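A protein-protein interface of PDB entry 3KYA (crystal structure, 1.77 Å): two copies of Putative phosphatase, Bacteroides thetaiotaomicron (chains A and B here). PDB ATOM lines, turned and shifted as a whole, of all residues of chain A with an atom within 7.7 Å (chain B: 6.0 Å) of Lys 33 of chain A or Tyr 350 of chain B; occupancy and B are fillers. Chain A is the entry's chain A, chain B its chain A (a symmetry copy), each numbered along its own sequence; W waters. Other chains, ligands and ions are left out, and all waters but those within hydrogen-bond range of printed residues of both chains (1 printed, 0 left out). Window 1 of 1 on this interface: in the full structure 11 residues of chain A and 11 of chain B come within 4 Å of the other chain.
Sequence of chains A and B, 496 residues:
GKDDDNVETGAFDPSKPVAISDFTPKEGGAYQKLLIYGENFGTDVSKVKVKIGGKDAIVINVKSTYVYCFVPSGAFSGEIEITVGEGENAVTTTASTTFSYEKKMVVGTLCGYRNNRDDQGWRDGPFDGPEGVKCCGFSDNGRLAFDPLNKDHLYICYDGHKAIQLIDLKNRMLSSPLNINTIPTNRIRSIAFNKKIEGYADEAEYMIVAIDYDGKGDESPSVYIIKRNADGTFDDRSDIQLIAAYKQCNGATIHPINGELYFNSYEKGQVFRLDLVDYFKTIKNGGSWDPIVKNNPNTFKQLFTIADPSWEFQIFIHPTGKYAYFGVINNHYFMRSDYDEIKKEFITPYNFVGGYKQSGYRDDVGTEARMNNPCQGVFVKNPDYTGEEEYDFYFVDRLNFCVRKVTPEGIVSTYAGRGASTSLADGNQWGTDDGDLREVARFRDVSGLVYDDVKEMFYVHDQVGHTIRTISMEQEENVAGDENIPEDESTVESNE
The side-chain carboxylate of Asp 338 of chain B lies within hydrogen-bond range of the side-chain hydroxyl of Tyr 68 of chain A (2.6 Å).
O of Tyr 68 of chain A is in hydrogen-bond range of N of Ile 60 of chain A, 2.8 Å away. The backbone NH (N) of Arg 336 of chain B sits at hydrogen-bond distance from the backbone carbonyl oxygen (O) of Tyr 350 of chain B. N of Thr 24 of chain A sits at hydrogen-bond distance from O of Leu 35 of chain A, at 2.9 Å. NH1 of Arg 336 of chain B is in salt-bridge range of OD1 of Asp 338 of chain B (2.8 Å). O of Asn 61 of chain A sits at hydrogen-bond distance from N of Tyr 68 of chain A, at 2.9 Å.
Among the printed residues, merely in contact across the chains: Lys 33 of chain A with Tyr 350 of chain B (3.7 Å), Leu 35 of chain A with Asp 338 of chain B (3.5 Å) and Tyr 68 of chain A with Tyr 350 of chain B (3.9 Å).
Lys 33 of chain A touches one residue of chain B. Of the printed residues of chain A, Tyr 350 of chain B touches Lys 33 and Tyr 68. Of the printed residues of chain A, Asp 338 of chain B touches Leu 35 (3.5 Å) and Tyr 68 (2.6 Å). Printed residues of chain B within 4 Å of Leu 35 of chain A: Asp 338 (3.5 Å). Of the printed residues of chain B, Tyr 68 of chain A touches Asp 338 (2.6 Å) and Tyr 350 (3.9 Å). Phe 70 of chain A touches none of the printed residues of chain B. Asn 351 of chain B touches none of the printed residues of chain A. The nearest printed residue of chain B that does not touch Lys 33 of chain A is Asn 351 of chain B (5.0 Å). The nearest printed residue of chain A that does not touch Tyr 350 of chain B is Asn 61 of chain A (6.9 Å). The nearest printed residue of chain A that does not touch Asp 338 of chain B is Thr 24 of chain A (4.9 Å).
Hydrophobic or aromatic side chains of chain A within 4 Å of the printed part of chain B: Leu 35 and Tyr 68. Of the 10 printed residues of chain B, 2 touch a printed residue of chain A. Printed residues of chain B that touch a printed residue of chain A: Asp 338 and Tyr 350. Hydrophobic or aromatic side chains of chain B within 4 Å of the printed part of chain A: Tyr 350. Among the printed residues, 4 pairs touch across the chains. Among the printed residues, no Asp or Glu carboxylate lies within 4 Å of a Lys or Arg side-chain nitrogen of the other chain.
No position is printed for both chains. Of the 4 pairs that touch across the chains among the printed residues, none has its exchanged pair printed and touching as well.
Water W1 lies within hydrogen-bond range of the side-chain hydroxyl of Tyr 68 of chain A, the backbone carbonyl oxygen of Thr 348 of chain B and the backbone NH of Asp 338 of chain B.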
ATOM      1  N   THR A  24      10.680 -13.178   1.148  1.00  0.00           N
ATOM      2  CA  THR A  24      10.299 -12.594  -0.120  1.00  0.00           C
ATOM      3  C   THR A  24      11.542 -12.251  -0.958  1.00  0.00           C
ATOM      4  O   THR A  24      12.531 -11.744  -0.418  1.00  0.00           O
ATOM      5  CB  THR A  24       9.416 -11.351   0.092  1.00  0.00           C
ATOM      6  OG1 THR A  24       8.914 -10.913  -1.168  1.00  0.00           O
ATOM      7  CG2 THR A  24      10.181 -10.218   0.761  1.00  0.00           C
ATOM      8  N   PRO A  25      11.509 -12.554  -2.269  1.00  0.00           N
ATOM      9  CA  PRO A  25      10.408 -13.201  -3.009  1.00  0.00           C
ATOM     10  C   PRO A  25      10.256 -14.690  -2.680  1.00  0.00           C
ATOM     11  O   PRO A  25      11.129 -15.277  -2.046  1.00  0.00           O
ATOM     12  CB  PRO A  25      10.815 -13.012  -4.471  1.00  0.00           C
ATOM     13  CG  PRO A  25      12.314 -13.001  -4.441  1.00  0.00           C
ATOM     14  CD  PRO A  25      12.671 -12.292  -3.138  1.00  0.00           C
ATOM     15  N   GLU A  27       9.956 -17.026  -4.984  1.00  0.00           N
ATOM     16  CA  GLU A  27      10.629 -17.733  -6.056  1.00  0.00           C
ATOM     17  C   GLU A  27      11.720 -16.837  -6.628  1.00  0.00           C
ATOM     18  O   GLU A  27      11.644 -15.611  -6.542  1.00  0.00           O
ATOM     19  CB  GLU A  27       9.641 -18.117  -7.170  1.00  0.00           C
ATOM     20  CG  GLU A  27       8.906 -16.930  -7.805  1.00  0.00           C
ATOM     21  CD  GLU A  27       7.799 -16.339  -6.921  1.00  0.00           C
ATOM     22  OE1 GLU A  27       6.826 -17.066  -6.593  1.00  0.00           O
ATOM     23  OE2 GLU A  27       7.868 -15.129  -6.585  1.00  0.00           O
ATOM     24  N   GLY A  29      16.003 -17.055  -8.812  1.00  0.00           N
ATOM     25  CA  GLY A  29      17.201 -17.788  -9.239  1.00  0.00           C
ATOM     26  C   GLY A  29      18.447 -17.386  -8.466  1.00  0.00           C
ATOM     27  O   GLY A  29      18.394 -16.533  -7.582  1.00  0.00           O
ATOM     28  N   ALA A  30      19.564 -18.026  -8.787  1.00  0.00           N
ATOM     29  CA  ALA A  30      20.844 -17.711  -8.158  1.00  0.00           C
ATOM     30  C   ALA A  30      21.143 -16.223  -8.278  1.00  0.00           C
ATOM     31  O   ALA A  30      20.811 -15.607  -9.275  1.00  0.00           O
ATOM     32  CB  ALA A  30      21.957 -18.525  -8.801  1.00  0.00           C
ATOM     33  N   TYR A  31      21.781 -15.664  -7.249  1.00  0.00           N
ATOM     34  CA  TYR A  31      22.138 -14.242  -7.155  1.00  0.00           C
ATOM     35  C   TYR A  31      20.961 -13.318  -6.792  1.00  0.00           C
ATOM     36  O   TYR A  31      21.161 -12.120  -6.637  1.00  0.00           O
ATOM     37  CB  TYR A  31      22.878 -13.725  -8.415  1.00  0.00           C
ATOM     38  CG  TYR A  31      24.205 -14.432  -8.652  1.00  0.00           C
ATOM     39  CD1 TYR A  31      24.265 -15.629  -9.368  1.00  0.00           C
ATOM     40  CD2 TYR A  31      25.396 -13.907  -8.139  1.00  0.00           C
ATOM     41  CE1 TYR A  31      25.481 -16.281  -9.584  1.00  0.00           C
ATOM     42  CE2 TYR A  31      26.620 -14.550  -8.346  1.00  0.00           C
ATOM     43  CZ  TYR A  31      26.657 -15.746  -9.066  1.00  0.00           C
ATOM     44  OH  TYR A  31      27.859 -16.401  -9.266  1.00  0.00           O
ATOM     45  N   GLN A  32      19.742 -13.858  -6.677  1.00  0.00           N
ATOM     46  CA  GLN A  32      18.593 -13.073  -6.226  1.00  0.00           C
ATOM     47  C   GLN A  32      18.810 -12.653  -4.781  1.00  0.00           C
ATOM     48  O   GLN A  32      19.271 -13.455  -3.966  1.00  0.00           O
ATOM     49  CB  GLN A  32      17.311 -13.917  -6.294  1.00  0.00           C
ATOM     50  CG  GLN A  32      16.063 -13.322  -5.605  1.00  0.00           C
ATOM     51  CD  GLN A  32      15.446 -12.133  -6.338  1.00  0.00           C
ATOM     52  OE1 GLN A  32      15.150 -11.078  -5.729  1.00  0.00           O
ATOM     53  NE2 GLN A  32      15.233 -12.297  -7.638  1.00  0.00           N
ATOM     54  N   LYS A  33      18.471 -11.407  -4.466  1.00  0.00           N
ATOM     55  CA  LYS A  33      18.514 -10.926  -3.097  1.00  0.00           C
ATOM     56  C   LYS A  33      17.238 -11.432  -2.409  1.00  0.00           C
ATOM     57  O   LYS A  33      16.126 -11.215  -2.914  1.00  0.00           O
ATOM     58  CB  LYS A  33      18.595  -9.412  -3.086  1.00  0.00           C
ATOM     59  CG  LYS A  33      18.946  -8.788  -1.779  1.00  0.00           C
ATOM     60  CD  LYS A  33      19.319  -7.307  -1.974  1.00  0.00           C
ATOM     61  CE  LYS A  33      20.647  -7.131  -2.749  1.00  0.00           C
ATOM     62  NZ  LYS A  33      21.142  -5.714  -2.843  1.00  0.00           N
ATOM     63  N   LEU A  34      17.401 -12.100  -1.272  1.00  0.00           N
ATOM     64  CA  LEU A  34      16.291 -12.672  -0.509  1.00  0.00           C
ATOM     65  C   LEU A  34      16.190 -12.048   0.880  1.00  0.00           C
ATOM     66  O   LEU A  34      17.191 -11.928   1.603  1.00  0.00           O
ATOM     67  CB  LEU A  34      16.475 -14.193  -0.379  1.00  0.00           C
ATOM     68  CG  LEU A  34      15.454 -14.983   0.431  1.00  0.00           C
ATOM     69  CD1 LEU A  34      14.100 -15.017  -0.304  1.00  0.00           C
ATOM     70  CD2 LEU A  34      15.984 -16.395   0.692  1.00  0.00           C
ATOM     71  N   LEU A  35      14.969 -11.676   1.247  1.00  0.00           N
ATOM     72  CA  LEU A  35      14.655 -11.076   2.534  1.00  0.00           C
ATOM     73  C   LEU A  35      13.927 -12.120   3.369  1.00  0.00           C
ATOM     74  O   LEU A  35      12.880 -12.633   2.955  1.00  0.00           O
ATOM     75  CB  LEU A  35      13.782  -9.824   2.344  1.00  0.00           C
ATOM     76  CG  LEU A  35      13.192  -9.158   3.591  1.00  0.00           C
ATOM     77  CD1 LEU A  35      14.269  -8.766   4.598  1.00  0.00           C
ATOM     78  CD2 LEU A  35      12.316  -7.922   3.240  1.00  0.00           C
ATOM     79  N   ILE A  36      14.500 -12.456   4.521  1.00  0.00           N
ATOM     80  CA  ILE A  36      13.934 -13.449   5.421  1.00  0.00           C
ATOM     81  C   ILE A  36      13.455 -12.775   6.705  1.00  0.00           C
ATOM     82  O   ILE A  36      14.223 -12.097   7.393  1.00  0.00           O
ATOM     83  CB  ILE A  36      14.965 -14.567   5.768  1.00  0.00           C
ATOM     84  CG1 ILE A  36      15.444 -15.301   4.511  1.00  0.00           C
ATOM     85  CG2 ILE A  36      14.357 -15.563   6.769  1.00  0.00           C
ATOM     86  CD1 ILE A  36      16.742 -16.118   4.737  1.00  0.00           C
ATOM     87  N   ILE A  60      24.061 -10.667   3.863  1.00  0.00           N
ATOM     88  CA  ILE A  60      24.279  -9.250   3.570  1.00  0.00           C
ATOM     89  C   ILE A  60      24.085  -8.336   4.775  1.00  0.00           C
ATOM     90  O   ILE A  60      24.915  -7.484   5.050  1.00  0.00           O
ATOM     91  CB  ILE A  60      23.314  -8.796   2.441  1.00  0.00           C
ATOM     92  CG1 ILE A  60      23.490  -9.653   1.183  1.00  0.00           C
ATOM     93  CG2 ILE A  60      23.498  -7.312   2.072  1.00  0.00           C
ATOM     94  CD1 ILE A  60      22.362  -9.493   0.154  1.00  0.00           C
ATOM     95  N   ASN A  61      22.995  -8.539   5.509  1.00  0.00           N
ATOM     96  CA  ASN A  61      22.639  -7.663   6.615  1.00  0.00           C
ATOM     97  C   ASN A  61      21.703  -8.414   7.552  1.00  0.00           C
ATOM     98  O   ASN A  61      20.858  -9.171   7.096  1.00  0.00           O
ATOM     99  CB  ASN A  61      21.962  -6.402   6.055  1.00  0.00           C
ATOM    100  CG  ASN A  61      21.701  -5.341   7.106  1.00  0.00           C
ATOM    101  OD1 ASN A  61      22.332  -5.315   8.166  1.00  0.00           O
ATOM    102  ND2 ASN A  61      20.770  -4.439   6.804  1.00  0.00           N
ATOM    103  N   VAL A  67      16.698 -10.845   7.908  1.00  0.00           N
ATOM    104  CA  VAL A  67      18.021 -11.098   7.355  1.00  0.00           C
ATOM    105  C   VAL A  67      17.948 -11.011   5.849  1.00  0.00           C
ATOM    106  O   VAL A  67      17.022 -11.551   5.236  1.00  0.00           O
ATOM    107  CB  VAL A  67      18.559 -12.504   7.730  1.00  0.00           C
ATOM    108  CG1 VAL A  67      19.920 -12.768   7.058  1.00  0.00           C
ATOM    109  CG2 VAL A  67      18.681 -12.647   9.236  1.00  0.00           C
ATOM    110  N   TYR A  68      18.925 -10.327   5.249  1.00  0.00           N
ATOM    111  CA  TYR A  68      19.057 -10.277   3.799  1.00  0.00           C
ATOM    112  C   TYR A  68      20.221 -11.175   3.405  1.00  0.00           C
ATOM    113  O   TYR A  68      21.269 -11.139   4.061  1.00  0.00           O
ATOM    114  CB  TYR A  68      19.388  -8.887   3.291  1.00  0.00           C
ATOM    115  CG  TYR A  68      18.239  -7.929   3.163  1.00  0.00           C
ATOM    116  CD1 TYR A  68      17.411  -7.959   2.049  1.00  0.00           C
ATOM    117  CD2 TYR A  68      18.023  -6.947   4.115  1.00  0.00           C
ATOM    118  CE1 TYR A  68      16.363  -7.045   1.907  1.00  0.00           C
ATOM    119  CE2 TYR A  68      16.982  -6.028   3.984  1.00  0.00           C
ATOM    120  CZ  TYR A  68      16.155  -6.091   2.877  1.00  0.00           C
ATOM    121  OH  TYR A  68      15.125  -5.176   2.744  1.00  0.00           O
ATOM    122  N   CYS A  69      20.031 -11.958   2.349  1.00  0.00           N
ATOM    123  CA  CYS A  69      21.086 -12.823   1.822  1.00  0.00           C
ATOM    124  C   CYS A  69      20.932 -12.979   0.309  1.00  0.00           C
ATOM    125  O   CYS A  69      19.945 -12.512  -0.289  1.00  0.00           O
ATOM    126  CB  CYS A  69      21.036 -14.188   2.508  1.00  0.00           C
ATOM    127  SG  CYS A  69      19.555 -15.154   2.100  1.00  0.00           S
ATOM    128  N   PHE A  70      21.926 -13.590  -0.325  1.00  0.00           N
ATOM    129  CA  PHE A  70      21.856 -13.892  -1.755  1.00  0.00           C
ATOM    130  C   PHE A  70      21.542 -15.361  -1.962  1.00  0.00           C
ATOM    131  O   PHE A  70      22.142 -16.230  -1.311  1.00  0.00           O
ATOM    132  CB  PHE A  70      23.187 -13.609  -2.454  1.00  0.00           C
ATOM    133  CG  PHE A  70      23.480 -12.148  -2.647  1.00  0.00           C
ATOM    134  CD1 PHE A  70      22.703 -11.387  -3.513  1.00  0.00           C
ATOM    135  CD2 PHE A  70      24.561 -11.544  -2.009  1.00  0.00           C
ATOM    136  CE1 PHE A  70      22.985 -10.036  -3.716  1.00  0.00           C
ATOM    137  CE2 PHE A  70      24.849 -10.186  -2.212  1.00  0.00           C
ATOM    138  CZ  PHE A  70      24.064  -9.442  -3.062  1.00  0.00           C
ATOM    139  N   VAL A  71      20.630 -15.655  -2.889  1.00  0.00           N
ATOM    140  CA  VAL A  71      20.307 -17.043  -3.217  1.00  0.00           C
ATOM    141  C   VAL A  71      21.509 -17.703  -3.905  1.00  0.00           C
ATOM    142  O   VAL A  71      21.994 -17.219  -4.921  1.00  0.00           O
ATOM    143  CB  VAL A  71      19.077 -17.142  -4.128  1.00  0.00           C
ATOM    144  CG1 VAL A  71      18.822 -18.591  -4.578  1.00  0.00           C
ATOM    145  CG2 VAL A  71      17.843 -16.546  -3.413  1.00  0.00           C
ATOM    146  N   PHE A  99      11.774 -22.215  -0.518  1.00  0.00           N
ATOM    147  CA  PHE A  99      11.934 -21.206  -1.558  1.00  0.00           C
ATOM    148  C   PHE A  99      11.832 -21.926  -2.896  1.00  0.00           C
ATOM    149  O   PHE A  99      12.322 -23.037  -3.022  1.00  0.00           O
ATOM    150  CB  PHE A  99      13.306 -20.538  -1.410  1.00  0.00           C
ATOM    151  CG  PHE A  99      13.630 -19.529  -2.478  1.00  0.00           C
ATOM    152  CD1 PHE A  99      13.105 -18.246  -2.432  1.00  0.00           C
ATOM    153  CD2 PHE A  99      14.523 -19.840  -3.484  1.00  0.00           C
ATOM    154  CE1 PHE A  99      13.428 -17.308  -3.399  1.00  0.00           C
ATOM    155  CE2 PHE A  99      14.853 -18.913  -4.450  1.00  0.00           C
ATOM    156  CZ  PHE A  99      14.298 -17.640  -4.410  1.00  0.00           C
ATOM    157  N   PHE B 334      19.113   6.077  -6.430  1.00  0.00           N
ATOM    158  CA  PHE B 334      17.906   5.570  -5.793  1.00  0.00           C
ATOM    159  C   PHE B 334      18.257   4.436  -4.825  1.00  0.00           C
ATOM    160  O   PHE B 334      19.137   3.591  -5.114  1.00  0.00           O
ATOM    161  CB  PHE B 334      16.878   4.976  -6.804  1.00  0.00           C
ATOM    162  CG  PHE B 334      16.111   5.989  -7.603  1.00  0.00           C
ATOM    163  CD1 PHE B 334      16.613   6.473  -8.797  1.00  0.00           C
ATOM    164  CD2 PHE B 334      14.838   6.399  -7.197  1.00  0.00           C
ATOM    165  CE1 PHE B 334      15.896   7.420  -9.537  1.00  0.00           C
ATOM    166  CE2 PHE B 334      14.133   7.338  -7.927  1.00  0.00           C
ATOM    167  CZ  PHE B 334      14.662   7.833  -9.104  1.00  0.00           C
ATOM    168  N   MET B 335      17.567   4.432  -3.689  1.00  0.00           N
ATOM    169  CA  MET B 335      17.628   3.358  -2.722  1.00  0.00           C
ATOM    170  C   MET B 335      16.291   2.606  -2.803  1.00  0.00           C
ATOM    171  O   MET B 335      15.297   3.141  -3.317  1.00  0.00           O
ATOM    172  CB  MET B 335      17.862   3.893  -1.307  1.00  0.00           C
ATOM    173  CG  MET B 335      19.131   4.726  -1.146  1.00  0.00           C
ATOM    174  SD  MET B 335      19.459   5.246   0.695  1.00  0.00           S
ATOM    175  CE  MET B 335      20.052   3.526   1.361  1.00  0.00           C
ATOM    176  N   ARG B 336      16.284   1.365  -2.330  1.00  0.00           N
ATOM    177  CA  ARG B 336      15.095   0.538  -2.305  1.00  0.00           C
ATOM    178  C   ARG B 336      14.809   0.129  -0.874  1.00  0.00           C
ATOM    179  O   ARG B 336      15.723  -0.217  -0.126  1.00  0.00           O
ATOM    180  CB  ARG B 336      15.264  -0.697  -3.172  1.00  0.00           C
ATOM    181  CG  ARG B 336      14.025  -1.592  -3.314  1.00  0.00           C
ATOM    182  CD  ARG B 336      14.368  -2.777  -4.226  1.00  0.00           C
ATOM    183  NE  ARG B 336      13.250  -3.669  -4.556  1.00  0.00           N
ATOM    184  CZ  ARG B 336      12.700  -4.531  -3.708  1.00  0.00           C
ATOM    185  NH1 ARG B 336      13.120  -4.592  -2.457  1.00  0.00           N
ATOM    186  NH2 ARG B 336      11.710  -5.317  -4.094  1.00  0.00           N
ATOM    187  N   SER B 337      13.529   0.152  -0.515  1.00  0.00           N
ATOM    188  CA  SER B 337      13.083  -0.238   0.811  1.00  0.00           C
ATOM    189  C   SER B 337      11.932  -1.255   0.732  1.00  0.00           C
ATOM    190  O   SER B 337      10.938  -1.014   0.034  1.00  0.00           O
ATOM    191  CB  SER B 337      12.653   1.028   1.563  1.00  0.00           C
ATOM    192  OG  SER B 337      12.102   0.749   2.828  1.00  0.00           O
ATOM    193  N   ASP B 338      12.064  -2.380   1.434  1.00  0.00           N
ATOM    194  CA  ASP B 338      10.997  -3.386   1.511  1.00  0.00           C
ATOM    195  C   ASP B 338       9.954  -2.995   2.571  1.00  0.00           C
ATOM    196  O   ASP B 338      10.280  -2.342   3.561  1.00  0.00           O
ATOM    197  CB  ASP B 338      11.564  -4.769   1.814  1.00  0.00           C
ATOM    198  CG  ASP B 338      12.303  -5.362   0.635  1.00  0.00           C
ATOM    199  OD1 ASP B 338      11.638  -5.643  -0.391  1.00  0.00           O
ATOM    200  OD2 ASP B 338      13.538  -5.550   0.724  1.00  0.00           O
ATOM    201  N   THR B 348      14.735  -0.314   6.812  1.00  0.00           N
ATOM    202  CA  THR B 348      15.962   0.341   6.391  1.00  0.00           C
ATOM    203  C   THR B 348      16.283   0.055   4.922  1.00  0.00           C
ATOM    204  O   THR B 348      16.387  -1.102   4.523  1.00  0.00           O
ATOM    205  CB  THR B 348      17.151  -0.087   7.277  1.00  0.00           C
ATOM    206  OG1 THR B 348      16.854   0.244   8.638  1.00  0.00           O
ATOM    207  CG2 THR B 348      18.414   0.620   6.853  1.00  0.00           C
ATOM    208  N   PRO B 349      16.422   1.115   4.112  1.00  0.00           N
ATOM    209  CA  PRO B 349      16.690   0.932   2.683  1.00  0.00           C
ATOM    210  C   PRO B 349      18.147   0.620   2.353  1.00  0.00           C
ATOM    211  O   PRO B 349      19.033   0.734   3.204  1.00  0.00           O
ATOM    212  CB  PRO B 349      16.301   2.294   2.082  1.00  0.00           C
ATOM    213  CG  PRO B 349      16.647   3.260   3.166  1.00  0.00           C
ATOM    214  CD  PRO B 349      16.234   2.543   4.448  1.00  0.00           C
ATOM    215  N   TYR B 350      18.374   0.227   1.106  1.00  0.00           N
ATOM    216  CA  TYR B 350      19.709  -0.077   0.610  1.00  0.00           C
ATOM    217  C   TYR B 350      19.900   0.517  -0.789  1.00  0.00           C
ATOM    218  O   TYR B 350      18.930   0.756  -1.513  1.00  0.00           O
ATOM    219  CB  TYR B 350      19.963  -1.596   0.620  1.00  0.00           C
ATOM    220  CG  TYR B 350      18.997  -2.452  -0.205  1.00  0.00           C
ATOM    221  CD1 TYR B 350      19.177  -2.619  -1.576  1.00  0.00           C
ATOM    222  CD2 TYR B 350      17.928  -3.123   0.396  1.00  0.00           C
ATOM    223  CE1 TYR B 350      18.319  -3.414  -2.326  1.00  0.00           C
ATOM    224  CE2 TYR B 350      17.066  -3.930  -0.350  1.00  0.00           C
ATOM    225  CZ  TYR B 350      17.267  -4.064  -1.709  1.00  0.00           C
ATOM    226  OH  TYR B 350      16.430  -4.860  -2.461  1.00  0.00           O
ATOM    227  N   ASN B 351      21.158   0.752  -1.153  1.00  0.00           N
ATOM    228  CA  ASN B 351      21.476   1.322  -2.460  1.00  0.00           C
ATOM    229  C   ASN B 351      20.993   0.386  -3.570  1.00  0.00           C
ATOM    230  O   ASN B 351      21.233  -0.810  -3.534  1.00  0.00           O
ATOM    231  CB  ASN B 351      22.969   1.641  -2.579  1.00  0.00           C
ATOM    232  CG  ASN B 351      23.422   2.691  -1.575  1.00  0.00           C
ATOM    233  OD1 ASN B 351      22.686   3.044  -0.656  1.00  0.00           O
ATOM    234  ND2 ASN B 351      24.654   3.174  -1.734  1.00  0.00           N
ATOM    235  N   PHE B 352      20.270   0.944  -4.538  1.00  0.00           N
ATOM    236  CA  PHE B 352      19.666   0.160  -5.629  1.00  0.00           C
ATOM    237  C   PHE B 352      20.247   0.470  -7.014  1.00  0.00           C
ATOM    238  O   PHE B 352      20.859  -0.409  -7.632  1.00  0.00           O
ATOM    239  CB  PHE B 352      18.128   0.343  -5.582  1.00  0.00           C
ATOM    240  CG  PHE B 352      17.383  -0.424  -6.659  1.00  0.00           C
ATOM    241  CD1 PHE B 352      17.565  -1.794  -6.816  1.00  0.00           C
ATOM    242  CD2 PHE B 352      16.477   0.224  -7.491  1.00  0.00           C
ATOM    243  CE1 PHE B 352      16.881  -2.493  -7.814  1.00  0.00           C
ATOM    244  CE2 PHE B 352      15.803  -0.470  -8.492  1.00  0.00           C
ATOM    245  CZ  PHE B 352      15.993  -1.823  -8.644  1.00  0.00           C
HETATM  246  O   HOH W   1      14.644  -2.457   2.775  1.00  0.00           O
